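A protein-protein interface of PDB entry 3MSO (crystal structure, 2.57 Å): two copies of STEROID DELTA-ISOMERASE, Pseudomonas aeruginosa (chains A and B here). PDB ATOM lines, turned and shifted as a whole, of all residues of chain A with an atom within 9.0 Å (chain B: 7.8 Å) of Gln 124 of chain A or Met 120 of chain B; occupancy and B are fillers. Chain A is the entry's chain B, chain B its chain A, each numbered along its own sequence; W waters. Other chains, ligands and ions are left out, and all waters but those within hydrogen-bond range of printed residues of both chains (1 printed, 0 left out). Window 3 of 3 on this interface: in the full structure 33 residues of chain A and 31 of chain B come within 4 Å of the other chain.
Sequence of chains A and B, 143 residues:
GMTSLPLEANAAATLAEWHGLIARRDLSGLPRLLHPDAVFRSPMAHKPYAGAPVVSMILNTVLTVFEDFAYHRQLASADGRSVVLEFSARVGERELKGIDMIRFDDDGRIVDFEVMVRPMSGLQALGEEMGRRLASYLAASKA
The backbone NH (N) of Met 44 of chain A lies close to the side-chain hydroxyl (OG) of Ser 42 of chain A (3.3 Å).
Water W1 lies within hydrogen-bond range of the backbone NH (N) of Val 117 of chain A (2.8 Å) and the backbone carbonyl oxygen (O) of Val 117 of chain B (3.1 Å).
O of Pro 43 of chain A touches CA of Pro 119 of chain B, at 3.4 Å. CB of Pro 119 of chain B touches O of Met 44 of chain A (3.5 Å). Ala 45 of chain A touches Pro 119 of chain B (C to CB, 3.5 Å). His 46 of chain A touches Pro 119 of chain B. CG of Met 116 of chain A touches CG of Arg 118 of chain B (3.7 Å). Pro 119 of chain A touches Met 44 of chain B (CB to O, 3.5 Å). Met 120 of chain A touches Gln 124 of chain B (CE to CG, 3.6 Å). Leu 123 of chain A touches Met 120 of chain B (CD2 to SD, 3.8 Å). CD2 of Leu 123 of chain A touches CD2 of Leu 123 of chain B, at 3.7 Å. Met 120 of chain B touches Gln 124 of chain A.
Of the 26 printed residues of chain A, 11 touch a printed residue of chain B. Along chain A the printed residues that touch a printed residue of chain B span positions 42 to 124. Of the 14 printed residues of chain B, 6 touch a printed residue of chain A. Printed residues of chain B that touch a printed residue of chain A: Met 44, Arg 118, Pro 119, Met 120, Leu 123 and Gln 124. Hydrophobic or aromatic side chains of chain B within 4 Å of the printed part of chain A: Pro 119, Met 120 and Leu 123.
Met 44 of chain A touches Met 120 of chain B, and with the chains exchanged Met 120 of chain A touches Met 44 of chain B. Met 120 of chain A touches its own counterpart, Met 120 of chain B. Met 120 of chain A touches Leu 123 of chain B, and with the chains exchanged Leu 123 of chain A touches Met 120 of chain B. Leu 123 of chain B touches its own counterpart, Leu 123 of chain A. Of the 19 pairs that touch across the chains among the printed residues, 10 have their exchanged pair printed and touching as well.
Gln 124 of chain A touches just one residue of chain B: Met 120. Met 120 of chain B touches just these residues of chain A: Pro 43 (3.3 Å), Met 44 (3.3 Å), Met 120 (3.1 Å), Leu 123 (3.8 Å) and Gln 124 (3.6 Å). Printed residues of chain A within 4 Å of Pro 119 of chain B: Pro 43 (3.4 Å), Met 44 (3.5 Å), Ala 45 (3.5 Å) and His 46 (3.8 Å). No residue of chain A comes within 4 Å of Ser 121 of chain B. No residue of chain A comes within 4 Å of Gly 122 of chain B. Of the printed residues of chain B, Leu 123 of chain A touches Met 120 and Leu 123. Printed residues of chain B within 4 Å of Pro 43 of chain A: Arg 118, Pro 119 and Met 120. Printed residues of chain B within 4 Å of Val 115 of chain A: Arg 118. The nearest printed residue of chain B that does not touch Ala 45 of chain A is Met 120 of chain B (4.9 Å).
The backbone carbonyl oxygen (O) of Pro 43 of chain A lies within hydrogen-bond range of the backbone NH (N) of Met 120 of chain B (3.3 Å). The guanidinium group of Arg 118 of chain B lies within hydrogen-bond range of the backbone carbonyl oxygen of Ser 42 of chain A. SD of Met 120 of chain A sits close to SD of Met 120 of chain B (3.1 Å). O of Met 44 of chain A lies within hydrogen-bond range of N of Met 120 of chain B (3.3 Å). NH2 of Arg 118 of chain B is in hydrogen-bond range of O of Ala 45 of chain A, 3.0 Å away. O of Met 44 of chain B lies within hydrogen-bond range of N of Met 120 of chain A (3.5 Å).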
ATOM      1  N   SER A  42       3.145 -11.817   1.956  1.00  0.00           N
ATOM      2  CA  SER A  42       1.900 -12.568   2.072  1.00  0.00           C
ATOM      3  C   SER A  42       0.940 -12.003   3.129  1.00  0.00           C
ATOM      4  O   SER A  42       1.378 -11.619   4.213  1.00  0.00           O
ATOM      5  CB  SER A  42       2.204 -14.035   2.378  1.00  0.00           C
ATOM      6  OG  SER A  42       1.043 -14.843   2.330  1.00  0.00           O
ATOM      7  N   PRO A  43      -0.386 -12.023   2.876  1.00  0.00           N
ATOM      8  CA  PRO A  43      -1.320 -11.620   3.942  1.00  0.00           C
ATOM      9  C   PRO A  43      -1.332 -12.636   5.091  1.00  0.00           C
ATOM     10  O   PRO A  43      -1.821 -12.326   6.172  1.00  0.00           O
ATOM     11  CB  PRO A  43      -2.675 -11.596   3.220  1.00  0.00           C
ATOM     12  CG  PRO A  43      -2.526 -12.553   2.085  1.00  0.00           C
ATOM     13  CD  PRO A  43      -1.107 -12.444   1.649  1.00  0.00           C
ATOM     14  N   MET A  44      -0.768 -13.836   4.845  1.00  0.00           N
ATOM     15  CA  MET A  44      -0.735 -14.978   5.742  1.00  0.00           C
ATOM     16  C   MET A  44       0.487 -15.059   6.627  1.00  0.00           C
ATOM     17  O   MET A  44       0.357 -15.441   7.793  1.00  0.00           O
ATOM     18  CB  MET A  44      -0.832 -16.269   4.911  1.00  0.00           C
ATOM     19  CG  MET A  44      -2.239 -16.585   4.414  1.00  0.00           C
ATOM     20  SD  MET A  44      -3.480 -16.912   5.924  1.00  0.00           S
ATOM     21  CE  MET A  44      -2.729 -18.532   6.676  1.00  0.00           C
ATOM     22  N   ALA A  45       1.682 -14.754   6.054  1.00  0.00           N
ATOM     23  CA  ALA A  45       3.010 -14.899   6.667  1.00  0.00           C
ATOM     24  C   ALA A  45       3.837 -13.633   6.806  1.00  0.00           C
ATOM     25  O   ALA A  45       3.751 -12.711   5.978  1.00  0.00           O
ATOM     26  CB  ALA A  45       3.817 -15.927   5.892  1.00  0.00           C
ATOM     27  N   HIS A  46       4.679 -13.655   7.861  1.00  0.00           N
ATOM     28  CA  HIS A  46       5.629 -12.645   8.295  1.00  0.00           C
ATOM     29  C   HIS A  46       6.802 -12.600   7.303  1.00  0.00           C
ATOM     30  O   HIS A  46       7.133 -11.527   6.786  1.00  0.00           O
ATOM     31  CB  HIS A  46       6.144 -13.066   9.676  1.00  0.00           C
ATOM     32  CG  HIS A  46       6.528 -11.954  10.607  1.00  0.00           C
ATOM     33  ND1 HIS A  46       5.619 -11.428  11.526  1.00  0.00           N
ATOM     34  CD2 HIS A  46       7.746 -11.396  10.834  1.00  0.00           C
ATOM     35  CE1 HIS A  46       6.302 -10.547  12.243  1.00  0.00           C
ATOM     36  NE2 HIS A  46       7.585 -10.486  11.861  1.00  0.00           N
ATOM     37  N   VAL A  65      -7.183 -18.908  -7.017  1.00  0.00           N
ATOM     38  CA  VAL A  65      -7.979 -19.022  -5.799  1.00  0.00           C
ATOM     39  C   VAL A  65      -9.110 -17.991  -5.760  1.00  0.00           C
ATOM     40  O   VAL A  65     -10.270 -18.371  -5.558  1.00  0.00           O
ATOM     41  CB  VAL A  65      -7.085 -19.003  -4.526  1.00  0.00           C
ATOM     42  CG1 VAL A  65      -7.927 -19.057  -3.256  1.00  0.00           C
ATOM     43  CG2 VAL A  65      -6.067 -20.139  -4.545  1.00  0.00           C
ATOM     44  N   VAL A  91     -13.847 -16.559  -1.743  1.00  0.00           N
ATOM     45  CA  VAL A  91     -13.184 -17.859  -1.663  1.00  0.00           C
ATOM     46  C   VAL A  91     -14.281 -18.783  -1.126  1.00  0.00           C
ATOM     47  O   VAL A  91     -14.557 -18.806   0.078  1.00  0.00           O
ATOM     48  CB  VAL A  91     -11.882 -17.822  -0.813  1.00  0.00           C
ATOM     49  CG1 VAL A  91     -11.282 -19.210  -0.677  1.00  0.00           C
ATOM     50  CG2 VAL A  91     -10.854 -16.873  -1.427  1.00  0.00           C
ATOM     51  N   ARG A  94     -16.842 -17.428   1.424  1.00  0.00           N
ATOM     52  CA  ARG A  94     -16.176 -16.303   2.049  1.00  0.00           C
ATOM     53  C   ARG A  94     -15.967 -15.110   1.178  1.00  0.00           C
ATOM     54  O   ARG A  94     -15.142 -15.101   0.265  1.00  0.00           O
ATOM     55  CB  ARG A  94     -14.933 -16.718   2.844  1.00  0.00           C
ATOM     56  CG  ARG A  94     -15.211 -16.904   4.341  1.00  0.00           C
ATOM     57  CD  ARG A  94     -16.341 -17.876   4.594  1.00  0.00           C
ATOM     58  NE  ARG A  94     -16.718 -17.965   6.002  1.00  0.00           N
ATOM     59  CZ  ARG A  94     -16.373 -18.961   6.803  1.00  0.00           C
ATOM     60  NH1 ARG A  94     -15.618 -19.956   6.349  1.00  0.00           N
ATOM     61  NH2 ARG A  94     -16.776 -18.973   8.065  1.00  0.00           N
ATOM     62  N   LEU A  96     -14.663 -11.536   0.522  1.00  0.00           N
ATOM     63  CA  LEU A  96     -13.512 -10.836   1.087  1.00  0.00           C
ATOM     64  C   LEU A  96     -13.201  -9.485   0.443  1.00  0.00           C
ATOM     65  O   LEU A  96     -13.698  -9.135  -0.629  1.00  0.00           O
ATOM     66  CB  LEU A  96     -12.257 -11.728   1.245  1.00  0.00           C
ATOM     67  CG  LEU A  96     -11.579 -12.220  -0.030  1.00  0.00           C
ATOM     68  CD1 LEU A  96     -10.585 -11.170  -0.627  1.00  0.00           C
ATOM     69  CD2 LEU A  96     -10.866 -13.513   0.214  1.00  0.00           C
ATOM     70  N   VAL A 115       0.273  -7.920  -0.013  1.00  0.00           N
ATOM     71  CA  VAL A 115      -1.176  -8.166  -0.034  1.00  0.00           C
ATOM     72  C   VAL A 115      -1.727  -8.206   1.398  1.00  0.00           C
ATOM     73  O   VAL A 115      -1.072  -8.740   2.287  1.00  0.00           O
ATOM     74  CB  VAL A 115      -1.518  -9.467  -0.828  1.00  0.00           C
ATOM     75  CG1 VAL A 115      -3.023  -9.746  -0.846  1.00  0.00           C
ATOM     76  CG2 VAL A 115      -0.970  -9.408  -2.250  1.00  0.00           C
ATOM     77  N   MET A 116      -2.911  -7.607   1.616  1.00  0.00           N
ATOM     78  CA  MET A 116      -3.668  -7.663   2.888  1.00  0.00           C
ATOM     79  C   MET A 116      -5.117  -8.026   2.522  1.00  0.00           C
ATOM     80  O   MET A 116      -5.639  -7.593   1.491  1.00  0.00           O
ATOM     81  CB  MET A 116      -3.665  -6.347   3.662  1.00  0.00           C
ATOM     82  CG  MET A 116      -2.278  -5.810   3.941  1.00  0.00           C
ATOM     83  SD  MET A 116      -2.338  -4.361   5.206  1.00  0.00           S
ATOM     84  CE  MET A 116      -0.528  -3.716   4.919  1.00  0.00           C
ATOM     85  N   VAL A 117      -5.739  -8.844   3.354  1.00  0.00           N
ATOM     86  CA  VAL A 117      -7.101  -9.315   3.158  1.00  0.00           C
ATOM     87  C   VAL A 117      -7.844  -9.147   4.482  1.00  0.00           C
ATOM     88  O   VAL A 117      -7.226  -9.201   5.548  1.00  0.00           O
ATOM     89  CB  VAL A 117      -7.091 -10.783   2.592  1.00  0.00           C
ATOM     90  CG1 VAL A 117      -8.393 -11.536   2.885  1.00  0.00           C
ATOM     91  CG2 VAL A 117      -6.787 -10.798   1.085  1.00  0.00           C
ATOM     92  N   ARG A 118      -9.148  -8.858   4.401  1.00  0.00           N
ATOM     93  CA  ARG A 118     -10.082  -8.758   5.529  1.00  0.00           C
ATOM     94  C   ARG A 118     -11.459  -9.329   5.087  1.00  0.00           C
ATOM     95  O   ARG A 118     -11.768  -9.252   3.888  1.00  0.00           O
ATOM     96  CB  ARG A 118     -10.186  -7.322   6.068  1.00  0.00           C
ATOM     97  CG  ARG A 118     -10.783  -6.311   5.093  1.00  0.00           C
ATOM     98  CD  ARG A 118     -11.234  -5.062   5.828  1.00  0.00           C
ATOM     99  NE  ARG A 118     -12.429  -5.315   6.636  1.00  0.00           N
ATOM    100  CZ  ARG A 118     -13.668  -5.228   6.171  1.00  0.00           C
ATOM    101  NH1 ARG A 118     -13.888  -4.877   4.912  1.00  0.00           N
ATOM    102  NH2 ARG A 118     -14.699  -5.481   6.965  1.00  0.00           N
ATOM    103  N   PRO A 119     -12.302  -9.887   5.990  1.00  0.00           N
ATOM    104  CA  PRO A 119     -12.100 -10.089   7.447  1.00  0.00           C
ATOM    105  C   PRO A 119     -11.298 -11.353   7.742  1.00  0.00           C
ATOM    106  O   PRO A 119     -10.854 -12.023   6.810  1.00  0.00           O
ATOM    107  CB  PRO A 119     -13.535 -10.179   7.972  1.00  0.00           C
ATOM    108  CG  PRO A 119     -14.282 -10.854   6.858  1.00  0.00           C
ATOM    109  CD  PRO A 119     -13.601 -10.439   5.558  1.00  0.00           C
ATOM    110  N   MET A 120     -11.129 -11.697   9.011  1.00  0.00           N
ATOM    111  CA  MET A 120     -10.419 -12.904   9.426  1.00  0.00           C
ATOM    112  C   MET A 120     -10.868 -14.156   8.630  1.00  0.00           C
ATOM    113  O   MET A 120     -10.019 -14.860   8.091  1.00  0.00           O
ATOM    114  CB  MET A 120     -10.621 -13.122  10.932  1.00  0.00           C
ATOM    115  CG  MET A 120     -10.105 -14.468  11.418  1.00  0.00           C
ATOM    116  SD  MET A 120      -8.183 -14.571  11.293  1.00  0.00           S
ATOM    117  CE  MET A 120      -7.898 -13.896  13.122  1.00  0.00           C
ATOM    118  N   SER A 121     -12.196 -14.410   8.556  1.00  0.00           N
ATOM    119  CA  SER A 121     -12.833 -15.537   7.849  1.00  0.00           C
ATOM    120  C   SER A 121     -12.376 -15.649   6.391  1.00  0.00           C
ATOM    121  O   SER A 121     -12.124 -16.765   5.919  1.00  0.00           O
ATOM    122  CB  SER A 121     -14.354 -15.433   7.926  1.00  0.00           C
ATOM    123  OG  SER A 121     -14.798 -14.094   7.761  1.00  0.00           O
ATOM    124  N   GLY A 122     -12.257 -14.503   5.716  1.00  0.00           N
ATOM    125  CA  GLY A 122     -11.798 -14.423   4.336  1.00  0.00           C
ATOM    126  C   GLY A 122     -10.337 -14.802   4.216  1.00  0.00           C
ATOM    127  O   GLY A 122      -9.972 -15.581   3.328  1.00  0.00           O
ATOM    128  N   LEU A 123      -9.486 -14.268   5.136  1.00  0.00           N
ATOM    129  CA  LEU A 123      -8.050 -14.556   5.203  1.00  0.00           C
ATOM    130  C   LEU A 123      -7.829 -16.048   5.447  1.00  0.00           C
ATOM    131  O   LEU A 123      -7.050 -16.663   4.717  1.00  0.00           O
ATOM    132  CB  LEU A 123      -7.373 -13.718   6.295  1.00  0.00           C
ATOM    133  CG  LEU A 123      -5.848 -13.852   6.460  1.00  0.00           C
ATOM    134  CD1 LEU A 123      -5.103 -13.461   5.194  1.00  0.00           C
ATOM    135  CD2 LEU A 123      -5.337 -13.045   7.677  1.00  0.00           C
ATOM    136  N   GLN A 124      -8.561 -16.637   6.414  1.00  0.00           N
ATOM    137  CA  GLN A 124      -8.498 -18.067   6.742  1.00  0.00           C
ATOM    138  C   GLN A 124      -8.758 -18.932   5.486  1.00  0.00           C
ATOM    139  O   GLN A 124      -7.973 -19.840   5.194  1.00  0.00           O
ATOM    140  CB  GLN A 124      -9.529 -18.425   7.821  1.00  0.00           C
ATOM    141  CG  GLN A 124      -9.286 -17.884   9.221  1.00  0.00           C
ATOM    142  CD  GLN A 124     -10.389 -18.333  10.161  1.00  0.00           C
ATOM    143  OE1 GLN A 124     -10.770 -17.660  11.128  1.00  0.00           O
ATOM    144  NE2 GLN A 124     -10.953 -19.484   9.884  1.00  0.00           N
ATOM    145  N   ALA A 125      -9.862 -18.625   4.747  1.00  0.00           N
ATOM    146  CA  ALA A 125     -10.270 -19.303   3.515  1.00  0.00           C
ATOM    147  C   ALA A 125      -9.171 -19.179   2.454  1.00  0.00           C
ATOM    148  O   ALA A 125      -8.781 -20.201   1.899  1.00  0.00           O
ATOM    149  CB  ALA A 125     -11.586 -18.723   3.006  1.00  0.00           C
ATOM    150  N   LEU A 126      -8.627 -17.955   2.228  1.00  0.00           N
ATOM    151  CA  LEU A 126      -7.530 -17.710   1.294  1.00  0.00           C
ATOM    152  C   LEU A 126      -6.310 -18.581   1.587  1.00  0.00           C
ATOM    153  O   LEU A 126      -5.894 -19.328   0.685  1.00  0.00           O
ATOM    154  CB  LEU A 126      -7.132 -16.218   1.240  1.00  0.00           C
ATOM    155  CG  LEU A 126      -5.907 -15.865   0.363  1.00  0.00           C
ATOM    156  CD1 LEU A 126      -6.156 -16.160  -1.121  1.00  0.00           C
ATOM    157  CD2 LEU A 126      -5.510 -14.424   0.567  1.00  0.00           C
ATOM    158  N   GLY A 127      -5.777 -18.491   2.816  1.00  0.00           N
ATOM    159  CA  GLY A 127      -4.648 -19.302   3.263  1.00  0.00           C
ATOM    160  C   GLY A 127      -4.853 -20.798   3.057  1.00  0.00           C
ATOM    161  O   GLY A 127      -3.987 -21.460   2.485  1.00  0.00           O
ATOM    162  N   GLU A 128      -6.031 -21.327   3.462  1.00  0.00           N
ATOM    163  CA  GLU A 128      -6.417 -22.732   3.326  1.00  0.00           C
ATOM    164  C   GLU A 128      -6.281 -23.183   1.863  1.00  0.00           C
ATOM    165  O   GLU A 128      -5.624 -24.189   1.588  1.00  0.00           O
ATOM    166  CB  GLU A 128      -7.877 -22.916   3.786  1.00  0.00           C
ATOM    167  CG  GLU A 128      -8.113 -23.875   4.930  1.00  0.00           C
ATOM    168  CD  GLU A 128      -9.030 -25.035   4.568  1.00  0.00           C
ATOM    169  OE1 GLU A 128      -8.717 -25.785   3.611  1.00  0.00           O
ATOM    170  OE2 GLU A 128     -10.032 -25.234   5.292  1.00  0.00           O
ATOM    171  N   GLU A 129      -6.885 -22.417   0.935  1.00  0.00           N
ATOM    172  CA  GLU A 129      -6.927 -22.694  -0.499  1.00  0.00           C
ATOM    173  C   GLU A 129      -5.577 -22.552  -1.179  1.00  0.00           C
ATOM    174  O   GLU A 129      -5.284 -23.337  -2.077  1.00  0.00           O
ATOM    175  CB  GLU A 129      -7.987 -21.824  -1.165  1.00  0.00           C
ATOM    176  CG  GLU A 129      -8.753 -22.523  -2.273  1.00  0.00           C
ATOM    177  CD  GLU A 129      -9.455 -23.814  -1.898  1.00  0.00           C
ATOM    178  OE1 GLU A 129     -10.248 -23.803  -0.931  1.00  0.00           O
ATOM    179  OE2 GLU A 129      -9.216 -24.838  -2.579  1.00  0.00           O
ATOM    180  N   MET A 130      -4.763 -21.559  -0.743  1.00  0.00           N
ATOM    181  CA  MET A 130      -3.414 -21.302  -1.255  1.00  0.00           C
ATOM    182  C   MET A 130      -2.561 -22.560  -1.037  1.00  0.00           C
ATOM    183  O   MET A 130      -1.887 -23.014  -1.958  1.00  0.00           O
ATOM    184  CB  MET A 130      -2.786 -20.076  -0.537  1.00  0.00           C
ATOM    185  CG  MET A 130      -2.291 -18.974  -1.489  1.00  0.00           C
ATOM    186  SD  MET A 130      -1.850 -17.227  -0.642  1.00  0.00           S
ATOM    187  CE  MET A 130       0.099 -17.475  -0.400  1.00  0.00           C
ATOM    188  N   GLY A 131      -2.628 -23.117   0.177  1.00  0.00           N
ATOM    189  CA  GLY A 131      -1.901 -24.315   0.600  1.00  0.00           C
ATOM    190  C   GLY A 131      -2.359 -25.570  -0.110  1.00  0.00           C
ATOM    191  O   GLY A 131      -1.535 -26.400  -0.512  1.00  0.00           O
ATOM    192  N   MET B  44     -11.309  -7.628  11.393  1.00  0.00           N
ATOM    193  CA  MET B  44     -11.797  -8.842  12.052  1.00  0.00           C
ATOM    194  C   MET B  44     -13.135  -9.347  11.559  1.00  0.00           C
ATOM    195  O   MET B  44     -13.327 -10.567  11.480  1.00  0.00           O
ATOM    196  CB  MET B  44     -11.900  -8.590  13.560  1.00  0.00           C
ATOM    197  CG  MET B  44     -10.541  -8.622  14.269  1.00  0.00           C
ATOM    198  SD  MET B  44      -9.639 -10.345  14.181  1.00  0.00           S
ATOM    199  CE  MET B  44     -10.905 -11.457  15.144  1.00  0.00           C
ATOM    200  N   ARG B  94       3.364  -9.812  18.828  1.00  0.00           N
ATOM    201  CA  ARG B  94       3.137  -9.795  17.396  1.00  0.00           C
ATOM    202  C   ARG B  94       3.368  -8.497  16.684  1.00  0.00           C
ATOM    203  O   ARG B  94       2.628  -7.531  16.872  1.00  0.00           O
ATOM    204  CB  ARG B  94       1.760 -10.395  17.046  1.00  0.00           C
ATOM    205  CG  ARG B  94       1.765 -11.881  16.662  1.00  0.00           C
ATOM    206  CD  ARG B  94       2.564 -12.728  17.619  1.00  0.00           C
ATOM    207  NE  ARG B  94       2.235 -14.147  17.601  1.00  0.00           N
ATOM    208  CZ  ARG B  94       2.881 -15.066  16.894  1.00  0.00           C
ATOM    209  NH1 ARG B  94       3.851 -14.709  16.053  1.00  0.00           N
ATOM    210  NH2 ARG B  94       2.552 -16.346  17.003  1.00  0.00           N
ATOM    211  N   LEU B  96       3.018  -6.384  13.483  1.00  0.00           N
ATOM    212  CA  LEU B  96       2.103  -6.406  12.373  1.00  0.00           C
ATOM    213  C   LEU B  96       2.347  -5.257  11.396  1.00  0.00           C
ATOM    214  O   LEU B  96       3.188  -4.376  11.611  1.00  0.00           O
ATOM    215  CB  LEU B  96       0.645  -6.512  12.856  1.00  0.00           C
ATOM    216  CG  LEU B  96       0.075  -5.345  13.678  1.00  0.00           C
ATOM    217  CD1 LEU B  96      -0.398  -4.185  12.788  1.00  0.00           C
ATOM    218  CD2 LEU B  96      -1.063  -5.806  14.517  1.00  0.00           C
ATOM    219  N   VAL B 117      -5.043  -5.674   8.362  1.00  0.00           N
ATOM    220  CA  VAL B 117      -3.832  -6.029   9.092  1.00  0.00           C
ATOM    221  C   VAL B 117      -3.294  -7.335   8.500  1.00  0.00           C
ATOM    222  O   VAL B 117      -4.058  -8.155   7.981  1.00  0.00           O
ATOM    223  CB  VAL B 117      -4.127  -6.087  10.637  1.00  0.00           C
ATOM    224  CG1 VAL B 117      -3.142  -6.956  11.391  1.00  0.00           C
ATOM    225  CG2 VAL B 117      -4.169  -4.677  11.242  1.00  0.00           C
ATOM    226  N   ARG B 118      -1.966  -7.466   8.498  1.00  0.00           N
ATOM    227  CA  ARG B 118      -1.224  -8.654   8.072  1.00  0.00           C
ATOM    228  C   ARG B 118       0.005  -8.820   8.985  1.00  0.00           C
ATOM    229  O   ARG B 118       0.500  -7.800   9.481  1.00  0.00           O
ATOM    230  CB  ARG B 118      -0.850  -8.595   6.573  1.00  0.00           C
ATOM    231  CG  ARG B 118       0.137  -7.509   6.191  1.00  0.00           C
ATOM    232  CD  ARG B 118       0.758  -7.777   4.840  1.00  0.00           C
ATOM    233  NE  ARG B 118       1.707  -8.888   4.909  1.00  0.00           N
ATOM    234  CZ  ARG B 118       2.988  -8.765   5.241  1.00  0.00           C
ATOM    235  NH1 ARG B 118       3.497  -7.576   5.525  1.00  0.00           N
ATOM    236  NH2 ARG B 118       3.772  -9.831   5.289  1.00  0.00           N
ATOM    237  N   PRO B 119       0.534 -10.049   9.234  1.00  0.00           N
ATOM    238  CA  PRO B 119       0.069 -11.368   8.768  1.00  0.00           C
ATOM    239  C   PRO B 119      -1.070 -11.916   9.631  1.00  0.00           C
ATOM    240  O   PRO B 119      -1.526 -11.231  10.540  1.00  0.00           O
ATOM    241  CB  PRO B 119       1.344 -12.209   8.874  1.00  0.00           C
ATOM    242  CG  PRO B 119       2.062 -11.650  10.060  1.00  0.00           C
ATOM    243  CD  PRO B 119       1.710 -10.185  10.120  1.00  0.00           C
ATOM    244  N   MET B 120      -1.490 -13.160   9.393  1.00  0.00           N
ATOM    245  CA  MET B 120      -2.537 -13.819  10.180  1.00  0.00           C
ATOM    246  C   MET B 120      -2.311 -13.677  11.696  1.00  0.00           C
ATOM    247  O   MET B 120      -3.226 -13.240  12.406  1.00  0.00           O
ATOM    248  CB  MET B 120      -2.644 -15.292   9.778  1.00  0.00           C
ATOM    249  CG  MET B 120      -3.540 -16.105  10.698  1.00  0.00           C
ATOM    250  SD  MET B 120      -5.401 -15.600  10.535  1.00  0.00           S
ATOM    251  CE  MET B 120      -5.785 -16.986   9.190  1.00  0.00           C
ATOM    252  N   SER B 121      -1.087 -14.022  12.168  1.00  0.00           N
ATOM    253  CA  SER B 121      -0.657 -13.948  13.572  1.00  0.00           C
ATOM    254  C   SER B 121      -0.908 -12.585  14.217  1.00  0.00           C
ATOM    255  O   SER B 121      -1.355 -12.527  15.374  1.00  0.00           O
ATOM    256  CB  SER B 121       0.817 -14.307  13.702  1.00  0.00           C
ATOM    257  OG  SER B 121       1.599 -13.748  12.663  1.00  0.00           O
ATOM    258  N   GLY B 122      -0.642 -11.517  13.456  1.00  0.00           N
ATOM    259  CA  GLY B 122      -0.857 -10.149  13.899  1.00  0.00           C
ATOM    260  C   GLY B 122      -2.327  -9.838  14.048  1.00  0.00           C
ATOM    261  O   GLY B 122      -2.731  -9.252  15.058  1.00  0.00           O
ATOM    262  N   LEU B 123      -3.140 -10.268  13.048  1.00  0.00           N
ATOM    263  CA  LEU B 123      -4.597 -10.099  13.033  1.00  0.00           C
ATOM    264  C   LEU B 123      -5.208 -10.807  14.229  1.00  0.00           C
ATOM    265  O   LEU B 123      -5.988 -10.192  14.959  1.00  0.00           O
ATOM    266  CB  LEU B 123      -5.213 -10.611  11.713  1.00  0.00           C
ATOM    267  CG  LEU B 123      -6.729 -10.410  11.510  1.00  0.00           C
ATOM    268  CD1 LEU B 123      -7.144  -8.935  11.577  1.00  0.00           C
ATOM    269  CD2 LEU B 123      -7.171 -10.982  10.187  1.00  0.00           C
ATOM    270  N   GLN B 124      -4.800 -12.063  14.463  1.00  0.00           N
ATOM    271  CA  GLN B 124      -5.256 -12.879  15.595  1.00  0.00           C
ATOM    272  C   GLN B 124      -5.040 -12.140  16.940  1.00  0.00           C
ATOM    273  O   GLN B 124      -5.977 -12.041  17.742  1.00  0.00           O
ATOM    274  CB  GLN B 124      -4.512 -14.232  15.642  1.00  0.00           C
ATOM    275  CG  GLN B 124      -4.834 -15.230  14.535  1.00  0.00           C
ATOM    276  CD  GLN B 124      -4.036 -16.501  14.724  1.00  0.00           C
ATOM    277  OE1 GLN B 124      -3.662 -17.198  13.776  1.00  0.00           O
ATOM    278  NE2 GLN B 124      -3.734 -16.825  15.965  1.00  0.00           N
ATOM    279  N   ALA B 125      -3.810 -11.628  17.164  1.00  0.00           N
ATOM    280  CA  ALA B 125      -3.426 -10.889  18.359  1.00  0.00           C
ATOM    281  C   ALA B 125      -4.295  -9.622  18.516  1.00  0.00           C
ATOM    282  O   ALA B 125      -4.854  -9.394  19.593  1.00  0.00           O
ATOM    283  CB  ALA B 125      -1.949 -10.535  18.293  1.00  0.00           C
ATOM    284  N   LEU B 126      -4.449  -8.833  17.430  1.00  0.00           N
ATOM    285  CA  LEU B 126      -5.296  -7.635  17.418  1.00  0.00           C
ATOM    286  C   LEU B 126      -6.746  -7.948  17.849  1.00  0.00           C
ATOM    287  O   LEU B 126      -7.250  -7.332  18.792  1.00  0.00           O
ATOM    288  CB  LEU B 126      -5.268  -6.926  16.052  1.00  0.00           C
ATOM    289  CG  LEU B 126      -6.174  -5.706  15.901  1.00  0.00           C
ATOM    290  CD1 LEU B 126      -5.729  -4.569  16.788  1.00  0.00           C
ATOM    291  CD2 LEU B 126      -6.240  -5.251  14.465  1.00  0.00           C
ATOM    292  N   GLY B 127      -7.363  -8.936  17.188  1.00  0.00           N
ATOM    293  CA  GLY B 127      -8.716  -9.394  17.476  1.00  0.00           C
ATOM    294  C   GLY B 127      -8.919  -9.841  18.904  1.00  0.00           C
ATOM    295  O   GLY B 127      -9.926  -9.485  19.522  1.00  0.00           O
HETATM  296  O   HOH W   1      -4.179  -9.843   5.442  1.00  0.00           O
